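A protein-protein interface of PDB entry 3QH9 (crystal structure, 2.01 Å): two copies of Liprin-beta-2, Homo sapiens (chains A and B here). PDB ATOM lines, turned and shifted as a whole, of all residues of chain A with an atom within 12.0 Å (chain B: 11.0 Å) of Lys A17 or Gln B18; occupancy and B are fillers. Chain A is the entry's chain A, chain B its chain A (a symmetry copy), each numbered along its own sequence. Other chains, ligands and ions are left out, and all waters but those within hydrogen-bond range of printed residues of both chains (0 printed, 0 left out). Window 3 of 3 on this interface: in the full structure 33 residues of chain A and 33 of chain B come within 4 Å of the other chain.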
ATOM      1  N   GLN A  14     -11.775  18.560   8.177  1.00  0.00           N
ATOM      2  CA  GLN A  14     -12.824  17.794   8.941  1.00  0.00           C
ATOM      3  C   GLN A  14     -12.501  17.633  10.470  1.00  0.00           C
ATOM      4  O   GLN A  14     -13.102  16.818  11.219  1.00  0.00           O
ATOM      5  CB  GLN A  14     -13.096  16.441   8.280  1.00  0.00           C
ATOM      6  CG  GLN A  14     -11.925  15.462   8.398  1.00  0.00           C
ATOM      7  CD  GLN A  14     -11.981  14.605   9.660  1.00  0.00           C
ATOM      8  OE1 GLN A  14     -11.161  14.768  10.584  1.00  0.00           O
ATOM      9  NE2 GLN A  14     -12.963  13.698   9.715  1.00  0.00           N
ATOM     10  N   GLU A  15     -11.570  18.447  10.939  1.00  0.00           N
ATOM     11  CA  GLU A  15     -11.592  18.804  12.332  1.00  0.00           C
ATOM     12  C   GLU A  15     -12.942  19.522  12.543  1.00  0.00           C
ATOM     13  O   GLU A  15     -13.520  19.455  13.631  1.00  0.00           O
ATOM     14  CB  GLU A  15     -10.396  19.686  12.716  1.00  0.00           C
ATOM     15  CG  GLU A  15     -10.347  21.058  12.015  1.00  0.00           C
ATOM     16  CD  GLU A  15     -10.063  22.218  12.976  1.00  0.00           C
ATOM     17  OE1 GLU A  15      -8.930  22.276  13.529  1.00  0.00           O
ATOM     18  OE2 GLU A  15     -10.980  23.066  13.158  1.00  0.00           O
ATOM     19  N   GLU A  16     -13.446  20.183  11.496  1.00  0.00           N
ATOM     20  CA  GLU A  16     -14.732  20.930  11.583  1.00  0.00           C
ATOM     21  C   GLU A  16     -16.018  20.063  11.589  1.00  0.00           C
ATOM     22  O   GLU A  16     -17.021  20.498  12.129  1.00  0.00           O
ATOM     23  CB  GLU A  16     -14.775  22.094  10.563  1.00  0.00           C
ATOM     24  CG  GLU A  16     -13.939  23.328  11.064  1.00  0.00           C
ATOM     25  CD  GLU A  16     -13.218  24.116   9.947  1.00  0.00           C
ATOM     26  OE1 GLU A  16     -13.927  24.780   9.151  1.00  0.00           O
ATOM     27  OE2 GLU A  16     -11.947  24.094   9.887  1.00  0.00           O
ATOM     28  N   LYS A  17     -15.956  18.855  11.018  1.00  0.00           N
ATOM     29  CA  LYS A  17     -16.898  17.762  11.344  1.00  0.00           C
ATOM     30  C   LYS A  17     -16.852  17.429  12.837  1.00  0.00           C
ATOM     31  O   LYS A  17     -17.901  17.287  13.502  1.00  0.00           O
ATOM     32  CB  LYS A  17     -16.510  16.474  10.620  1.00  0.00           C
ATOM     33  CG  LYS A  17     -17.669  15.661  10.020  1.00  0.00           C
ATOM     34  CD  LYS A  17     -17.796  15.902   8.495  1.00  0.00           C
ATOM     35  CE  LYS A  17     -17.941  14.604   7.715  1.00  0.00           C
ATOM     36  NZ  LYS A  17     -18.564  14.861   6.377  1.00  0.00           N
ATOM     37  N   GLN A  18     -15.628  17.259  13.348  1.00  0.00           N
ATOM     38  CA  GLN A  18     -15.426  17.053  14.778  1.00  0.00           C
ATOM     39  C   GLN A  18     -15.951  18.259  15.583  1.00  0.00           C
ATOM     40  O   GLN A  18     -16.674  18.078  16.569  1.00  0.00           O
ATOM     41  CB  GLN A  18     -13.953  16.738  15.090  1.00  0.00           C
ATOM     42  CG  GLN A  18     -13.645  16.410  16.567  1.00  0.00           C
ATOM     43  CD  GLN A  18     -14.515  15.284  17.127  1.00  0.00           C
ATOM     44  OE1 GLN A  18     -14.581  14.197  16.559  1.00  0.00           O
ATOM     45  NE2 GLN A  18     -15.161  15.538  18.261  1.00  0.00           N
ATOM     46  N   ARG A  19     -15.621  19.470  15.149  1.00  0.00           N
ATOM     47  CA  ARG A  19     -16.001  20.679  15.863  1.00  0.00           C
ATOM     48  C   ARG A  19     -17.499  20.887  15.876  1.00  0.00           C
ATOM     49  O   ARG A  19     -18.077  21.213  16.933  1.00  0.00           O
ATOM     50  CB  ARG A  19     -15.341  21.872  15.219  1.00  0.00           C
ATOM     51  CG  ARG A  19     -15.285  23.180  15.992  1.00  0.00           C
ATOM     52  CD  ARG A  19     -14.736  24.188  14.977  1.00  0.00           C
ATOM     53  NE  ARG A  19     -14.035  25.378  15.454  1.00  0.00           N
ATOM     54  CZ  ARG A  19     -14.406  26.172  16.458  1.00  0.00           C
ATOM     55  NH1 ARG A  19     -15.494  25.928  17.183  1.00  0.00           N
ATOM     56  NH2 ARG A  19     -13.659  27.238  16.740  1.00  0.00           N
ATOM     57  N   LYS A  20     -18.145  20.701  14.728  1.00  0.00           N
ATOM     58  CA  LYS A  20     -19.590  20.759  14.699  1.00  0.00           C
ATOM     59  C   LYS A  20     -20.215  19.657  15.564  1.00  0.00           C
ATOM     60  O   LYS A  20     -21.264  19.882  16.173  1.00  0.00           O
ATOM     61  CB  LYS A  20     -20.112  20.666  13.265  1.00  0.00           C
ATOM     62  CG  LYS A  20     -21.642  20.631  13.131  1.00  0.00           C
ATOM     63  CD  LYS A  20     -22.305  21.998  13.425  1.00  0.00           C
ATOM     64  CE  LYS A  20     -23.822  21.979  13.105  1.00  0.00           C
ATOM     65  NZ  LYS A  20     -24.176  21.871  11.630  1.00  0.00           N
ATOM     66  N   ALA A  21     -19.596  18.467  15.604  1.00  0.00           N
ATOM     67  CA  ALA A  21     -20.083  17.389  16.486  1.00  0.00           C
ATOM     68  C   ALA A  21     -20.104  17.900  17.913  1.00  0.00           C
ATOM     69  O   ALA A  21     -21.129  17.814  18.593  1.00  0.00           O
ATOM     70  CB  ALA A  21     -19.253  16.115  16.387  1.00  0.00           C
ATOM     71  N   GLU A  22     -19.001  18.497  18.342  1.00  0.00           N
ATOM     72  CA  GLU A  22     -18.896  18.869  19.766  1.00  0.00           C
ATOM     73  C   GLU A  22     -19.874  20.007  20.144  1.00  0.00           C
ATOM     74  O   GLU A  22     -20.371  20.029  21.264  1.00  0.00           O
ATOM     75  CB  GLU A  22     -17.443  19.149  20.198  1.00  0.00           C
ATOM     76  CG  GLU A  22     -16.532  17.958  20.057  1.00  0.00           C
ATOM     77  CD  GLU A  22     -15.058  18.284  20.362  1.00  0.00           C
ATOM     78  OE1 GLU A  22     -14.794  19.285  21.078  1.00  0.00           O
ATOM     79  OE2 GLU A  22     -14.172  17.543  19.911  1.00  0.00           O
ATOM     80  N   GLU A  23     -20.164  20.877  19.170  1.00  0.00           N
ATOM     81  CA  GLU A  23     -21.136  21.970  19.274  1.00  0.00           C
ATOM     82  C   GLU A  23     -22.528  21.445  19.546  1.00  0.00           C
ATOM     83  O   GLU A  23     -23.172  21.884  20.482  1.00  0.00           O
ATOM     84  CB  GLU A  23     -21.160  22.800  17.988  1.00  0.00           C
ATOM     85  CG  GLU A  23     -20.172  24.009  18.042  1.00  0.00           C
ATOM     86  CD  GLU A  23     -19.653  24.505  16.667  1.00  0.00           C
ATOM     87  OE1 GLU A  23     -18.808  25.438  16.645  1.00  0.00           O
ATOM     88  OE2 GLU A  23     -20.065  23.966  15.616  1.00  0.00           O
ATOM     89  N   LEU A  24     -22.960  20.515  18.698  1.00  0.00           N
ATOM     90  CA  LEU A  24     -24.170  19.721  18.877  1.00  0.00           C
ATOM     91  C   LEU A  24     -24.293  18.964  20.209  1.00  0.00           C
ATOM     92  O   LEU A  24     -25.363  18.926  20.740  1.00  0.00           O
ATOM     93  CB  LEU A  24     -24.364  18.790  17.660  1.00  0.00           C
ATOM     94  CG  LEU A  24     -25.333  19.335  16.566  1.00  0.00           C
ATOM     95  CD1 LEU A  24     -25.547  20.896  16.594  1.00  0.00           C
ATOM     96  CD2 LEU A  24     -24.908  18.848  15.171  1.00  0.00           C
ATOM     97  N   LEU A  25     -23.199  18.457  20.800  1.00  0.00           N
ATOM     98  CA  LEU A  25     -23.305  17.728  22.067  1.00  0.00           C
ATOM     99  C   LEU A  25     -23.653  18.679  23.193  1.00  0.00           C
ATOM    100  O   LEU A  25     -24.496  18.378  24.025  1.00  0.00           O
ATOM    101  CB  LEU A  25     -22.010  17.014  22.372  1.00  0.00           C
ATOM    102  CG  LEU A  25     -21.770  15.723  21.624  1.00  0.00           C
ATOM    103  CD1 LEU A  25     -20.352  15.199  21.954  1.00  0.00           C
ATOM    104  CD2 LEU A  25     -22.818  14.751  22.036  1.00  0.00           C
ATOM    105  N   GLN A  26     -22.971  19.821  23.169  1.00  0.00           N
ATOM    106  CA  GLN A  26     -23.150  20.957  24.068  1.00  0.00           C
ATOM    107  C   GLN A  26     -24.581  21.404  24.037  1.00  0.00           C
ATOM    108  O   GLN A  26     -25.229  21.591  25.064  1.00  0.00           O
ATOM    109  CB  GLN A  26     -22.247  22.122  23.612  1.00  0.00           C
ATOM    110  CG  GLN A  26     -22.196  23.341  24.576  1.00  0.00           C
ATOM    111  CD  GLN A  26     -21.054  24.365  24.279  1.00  0.00           C
ATOM    112  OE1 GLN A  26     -20.551  24.496  23.136  1.00  0.00           O
ATOM    113  NE2 GLN A  26     -20.655  25.103  25.331  1.00  0.00           N
ATOM    114  N   GLN B  14     -15.033   7.552   8.434  1.00  0.00           N
ATOM    115  CA  GLN B  14     -15.628   8.835   8.955  1.00  0.00           C
ATOM    116  C   GLN B  14     -16.913   9.298   8.179  1.00  0.00           C
ATOM    117  O   GLN B  14     -17.400  10.455   8.282  1.00  0.00           O
ATOM    118  CB  GLN B  14     -14.572   9.941   9.003  1.00  0.00           C
ATOM    119  CG  GLN B  14     -14.124  10.411   7.617  1.00  0.00           C
ATOM    120  CD  GLN B  14     -14.972  11.553   7.064  1.00  0.00           C
ATOM    121  OE1 GLN B  14     -15.739  11.373   6.098  1.00  0.00           O
ATOM    122  NE2 GLN B  14     -14.855  12.731   7.685  1.00  0.00           N
ATOM    123  N   GLU B  15     -17.484   8.371   7.428  1.00  0.00           N
ATOM    124  CA  GLU B  15     -18.892   8.464   7.155  1.00  0.00           C
ATOM    125  C   GLU B  15     -19.577   8.385   8.536  1.00  0.00           C
ATOM    126  O   GLU B  15     -20.646   8.969   8.736  1.00  0.00           O
ATOM    127  CB  GLU B  15     -19.366   7.355   6.206  1.00  0.00           C
ATOM    128  CG  GLU B  15     -19.221   5.921   6.755  1.00  0.00           C
ATOM    129  CD  GLU B  15     -20.477   5.067   6.555  1.00  0.00           C
ATOM    130  OE1 GLU B  15     -20.814   4.758   5.378  1.00  0.00           O
ATOM    131  OE2 GLU B  15     -21.111   4.705   7.586  1.00  0.00           O
ATOM    132  N   GLU B  16     -18.948   7.684   9.485  1.00  0.00           N
ATOM    133  CA  GLU B  16     -19.519   7.522  10.851  1.00  0.00           C
ATOM    134  C   GLU B  16     -19.423   8.761  11.777  1.00  0.00           C
ATOM    135  O   GLU B  16     -20.246   8.900  12.666  1.00  0.00           O
ATOM    136  CB  GLU B  16     -19.021   6.214  11.515  1.00  0.00           C
ATOM    137  CG  GLU B  16     -19.791   4.960  10.962  1.00  0.00           C
ATOM    138  CD  GLU B  16     -18.937   3.677  10.847  1.00  0.00           C
ATOM    139  OE1 GLU B  16     -18.572   3.121  11.913  1.00  0.00           O
ATOM    140  OE2 GLU B  16     -18.659   3.212   9.696  1.00  0.00           O
ATOM    141  N   LYS B  17     -18.446   9.643  11.535  1.00  0.00           N
ATOM    142  CA  LYS B  17     -18.502  11.051  11.990  1.00  0.00           C
ATOM    143  C   LYS B  17     -19.737  11.757  11.427  1.00  0.00           C
ATOM    144  O   LYS B  17     -20.470  12.459  12.157  1.00  0.00           O
ATOM    145  CB  LYS B  17     -17.301  11.839  11.470  1.00  0.00           C
ATOM    146  CG  LYS B  17     -16.650  12.810  12.467  1.00  0.00           C
ATOM    147  CD  LYS B  17     -15.365  12.206  13.086  1.00  0.00           C
ATOM    148  CE  LYS B  17     -14.199  13.184  13.067  1.00  0.00           C
ATOM    149  NZ  LYS B  17     -13.175  12.801  14.092  1.00  0.00           N
ATOM    150  N   GLN B  18     -19.936  11.604  10.114  1.00  0.00           N
ATOM    151  CA  GLN B  18     -21.134  12.124   9.464  1.00  0.00           C
ATOM    152  C   GLN B  18     -22.402  11.480  10.062  1.00  0.00           C
ATOM    153  O   GLN B  18     -23.359  12.191  10.391  1.00  0.00           O
ATOM    154  CB  GLN B  18     -21.055  11.951   7.937  1.00  0.00           C
ATOM    155  CG  GLN B  18     -22.233  12.552   7.141  1.00  0.00           C
ATOM    156  CD  GLN B  18     -22.479  14.030   7.454  1.00  0.00           C
ATOM    157  OE1 GLN B  18     -21.571  14.852   7.363  1.00  0.00           O
ATOM    158  NE2 GLN B  18     -23.718  14.368   7.796  1.00  0.00           N
ATOM    159  N   ARG B  19     -22.394  10.164  10.231  1.00  0.00           N
ATOM    160  CA  ARG B  19     -23.556   9.439  10.723  1.00  0.00           C
ATOM    161  C   ARG B  19     -23.897   9.809  12.149  1.00  0.00           C
ATOM    162  O   ARG B  19     -25.081  10.037  12.471  1.00  0.00           O
ATOM    163  CB  ARG B  19     -23.293   7.957  10.646  1.00  0.00           C
ATOM    164  CG  ARG B  19     -24.471   7.002  10.751  1.00  0.00           C
ATOM    165  CD  ARG B  19     -23.820   5.617  10.827  1.00  0.00           C
ATOM    166  NE  ARG B  19     -24.575   4.443  10.392  1.00  0.00           N
ATOM    167  CZ  ARG B  19     -25.848   4.166  10.674  1.00  0.00           C
ATOM    168  NH1 ARG B  19     -26.605   4.990  11.393  1.00  0.00           N
ATOM    169  NH2 ARG B  19     -26.372   3.029  10.217  1.00  0.00           N
ATOM    170  N   LYS B  20     -22.888   9.881  13.013  1.00  0.00           N
ATOM    171  CA  LYS B  20     -23.127  10.352  14.360  1.00  0.00           C
ATOM    172  C   LYS B  20     -23.618  11.806  14.368  1.00  0.00           C
ATOM    173  O   LYS B  20     -24.435  12.166  15.219  1.00  0.00           O
ATOM    174  CB  LYS B  20     -21.869  10.214  15.218  1.00  0.00           C
ATOM    175  CG  LYS B  20     -21.991  10.769  16.645  1.00  0.00           C
ATOM    176  CD  LYS B  20     -22.875   9.887  17.561  1.00  0.00           C
ATOM    177  CE  LYS B  20     -22.831  10.369  19.034  1.00  0.00           C
ATOM    178  NZ  LYS B  20     -21.501  10.170  19.746  1.00  0.00           N
ATOM    179  N   ALA B  21     -23.113  12.641  13.450  1.00  0.00           N
ATOM    180  CA  ALA B  21     -23.606  14.028  13.334  1.00  0.00           C
ATOM    181  C   ALA B  21     -25.102  13.994  13.095  1.00  0.00           C
ATOM    182  O   ALA B  21     -25.865  14.642  13.814  1.00  0.00           O
ATOM    183  CB  ALA B  21     -22.907  14.822  12.236  1.00  0.00           C
ATOM    184  N   GLU B  22     -25.527  13.184  12.135  1.00  0.00           N
ATOM    185  CA  GLU B  22     -26.949  13.226  11.741  1.00  0.00           C
ATOM    186  C   GLU B  22     -27.878  12.686  12.855  1.00  0.00           C
ATOM    187  O   GLU B  22     -28.995  13.172  12.998  1.00  0.00           O
ATOM    188  CB  GLU B  22     -27.202  12.569  10.370  1.00  0.00           C
ATOM    189  CG  GLU B  22     -26.481  13.247   9.234  1.00  0.00           C
ATOM    190  CD  GLU B  22     -26.631  12.505   7.893  1.00  0.00           C
ATOM    191  OE1 GLU B  22     -27.609  11.729   7.736  1.00  0.00           O
ATOM    192  OE2 GLU B  22     -25.797  12.705   6.998  1.00  0.00           O
ATOM    193  N   GLU B  23     -27.356  11.743  13.648  1.00  0.00           N
ATOM    194  CA  GLU B  23     -28.016  11.164  14.821  1.00  0.00           C
ATOM    195  C   GLU B  23     -28.307  12.218  15.867  1.00  0.00           C
ATOM    196  O   GLU B  23     -29.434  12.334  16.316  1.00  0.00           O
ATOM    197  CB  GLU B  23     -27.149  10.069  15.448  1.00  0.00           C
ATOM    198  CG  GLU B  23     -27.476   8.651  14.876  1.00  0.00           C
ATOM    199  CD  GLU B  23     -26.313   7.628  14.934  1.00  0.00           C
ATOM    200  OE1 GLU B  23     -26.493   6.486  14.436  1.00  0.00           O
ATOM    201  OE2 GLU B  23     -25.223   7.954  15.456  1.00  0.00           O
ATOM    202  N   LEU B  24     -27.262  12.956  16.235  1.00  0.00           N
ATOM    203  CA  LEU B  24     -27.339  14.153  17.063  1.00  0.00           C
ATOM    204  C   LEU B  24     -28.301  15.252  16.579  1.00  0.00           C
ATOM    205  O   LEU B  24     -28.953  15.830  17.396  1.00  0.00           O
ATOM    206  CB  LEU B  24     -25.917  14.699  17.318  1.00  0.00           C
ATOM    207  CG  LEU B  24     -25.280  14.259  18.673  1.00  0.00           C
ATOM    208  CD1 LEU B  24     -25.915  12.965  19.309  1.00  0.00           C
ATOM    209  CD2 LEU B  24     -23.754  14.132  18.540  1.00  0.00           C
ATOM    210  N   LEU B  25     -28.470  15.467  15.264  1.00  0.00           N
ATOM    211  CA  LEU B  25     -29.379  16.516  14.792  1.00  0.00           C
ATOM    212  C   LEU B  25     -30.817  16.126  15.063  1.00  0.00           C
ATOM    213  O   LEU B  25     -31.609  16.942  15.512  1.00  0.00           O
ATOM    214  CB  LEU B  25     -29.177  16.759  13.316  1.00  0.00           C
ATOM    215  CG  LEU B  25     -27.978  17.598  12.938  1.00  0.00           C
ATOM    216  CD1 LEU B  25     -27.848  17.635  11.396  1.00  0.00           C
ATOM    217  CD2 LEU B  25     -28.175  18.961  13.499  1.00  0.00           C
ATOM    218  N   GLN B  26     -31.100  14.859  14.775  1.00  0.00           N
ATOM    219  CA  GLN B  26     -32.369  14.178  15.009  1.00  0.00           C
ATOM    220  C   GLN B  26     -32.746  14.299  16.456  1.00  0.00           C
ATOM    221  O   GLN B  26     -33.864  14.667  16.810  1.00  0.00           O
ATOM    222  CB  GLN B  26     -32.227  12.685  14.648  1.00  0.00           C
ATOM    223  CG  GLN B  26     -33.548  11.865  14.677  1.00  0.00           C
ATOM    224  CD  GLN B  26     -33.460  10.455  14.012  1.00  0.00           C
ATOM    225  OE1 GLN B  26     -32.378   9.824  13.914  1.00  0.00           O
ATOM    226  NE2 GLN B  26     -34.626   9.957  13.560  1.00  0.00           N
ATOM    227  N   ARG B  29     -33.596  17.946  17.209  1.00  0.00           N
ATOM    228  CA  ARG B  29     -34.921  18.249  16.712  1.00  0.00           C
ATOM    229  C   ARG B  29     -35.978  17.746  17.675  1.00  0.00           C
ATOM    230  O   ARG B  29     -36.955  18.463  17.927  1.00  0.00           O
ATOM    231  CB  ARG B  29     -35.205  17.591  15.319  1.00  0.00           C
ATOM    232  CG  ARG B  29     -34.362  18.078  14.140  1.00  0.00           C
ATOM    233  CD  ARG B  29     -34.793  17.406  12.751  1.00  0.00           C
ATOM    234  NE  ARG B  29     -34.448  15.963  12.596  1.00  0.00           N
ATOM    235  CZ  ARG B  29     -33.384  15.447  11.939  1.00  0.00           C
ATOM    236  NH1 ARG B  29     -32.473  16.215  11.323  1.00  0.00           N
ATOM    237  NH2 ARG B  29     -33.222  14.118  11.899  1.00  0.00           N
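The side-chain carboxylate (OE2) of Glu A22 is in hydrogen-bond range of the side-chain amide nitrogen (NE2) of Gln A18, at 2.8 Å. The side-chain amide nitrogen (NE2) of Gln B18 is in hydrogen-bond range of the side-chain carboxylate (OE2) of Glu B22 (2.8 Å).
Gln A14 touches its own counterpart, Gln B14. Lys B17 touches its own counterpart, Lys A17. Lys A17 touches Gln B18, and with the chains exchanged Gln A18 touches Lys B17. Leu A24 touches Leu B25, and with the chains exchanged Leu A25 touches Leu B24. Of the 8 pairs that touch across the chains among the printed residues, 8 have their exchanged pair printed and touching as well.
Printed residues of chain B that touch a printed residue of chain A: Gln B14, Lys B17, Gln B18, Leu B24 and Leu B25. Hydrophobic or aromatic side chains of chain A within 4 Å of the printed part of chain B: Leu A24 and Leu A25. Along chain A the printed residues that touch a printed residue of chain B span positions 14 to 25. Among the printed residues, 8 pairs touch across the chains. Among the printed residues, no Asp or Glu carboxylate lies within 4 Å of a Lys or Arg side-chain nitrogen of the other chain.
Lys A17 touches just these residues of chain B: Gln B14 (3.6 Å), Lys B17 (3.9 Å) and Gln B18 (3.2 Å). Gln B18 touches just one residue of chain A: Lys A17 (3.2 Å). No residue of chain B comes within 4 Å of Glu A16. Of chain B, only Lys B17 comes within 4 Å of Gln A18. No residue of chain B comes within 4 Å of Ala A21. Gln B14 touches just these residues of chain A: Gln A14 and Lys A17. No residue of chain A comes within 4 Å of Glu B15. No residue of chain A comes within 4 Å of Ala B21. No residue of chain A comes within 4 Å of Glu B22. Printed residues of chain B within 4 Å of Leu A25: Leu B24. Printed residues of chain A within 4 Å of Leu B25: Leu A24 (3.7 Å). Printed residues of chain B within 4 Å of Leu A24: Leu B25. Printed residues of chain A within 4 Å of Leu B24: Leu A25. Lys A20 touches none of the printed residues of chain B. The nearest residue of chain B that does not touch Lys A17 is Ala B21 (5.7 Å). The nearest printed residue of chain B that does not touch Leu A24 is Leu B24 (4.4 Å).
Among the printed residues, pairs that only touch across the chains: Gln A14 with Lys B17 (3.6 Å), Lys A17 with Gln B14 (3.6 Å), Lys A17 with Lys B17 (3.9 Å), Leu A24 with Leu B25 (3.7 Å) and Leu A25 with Leu B24 (3.7 Å).
The side-chain amide nitrogen (NE2) of Gln B14 lies close to the side-chain amide nitrogen (NE2) of Gln A14 (2.9 Å). The side-chain amide oxygen (OE1) of Gln B18 lies within hydrogen-bond range of the side-chain amino group (NZ) of Lys A17, 3.2 Å away. OE1 of Gln A18 lies within hydrogen-bond range of NZ of Lys B17 (3.2 Å).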
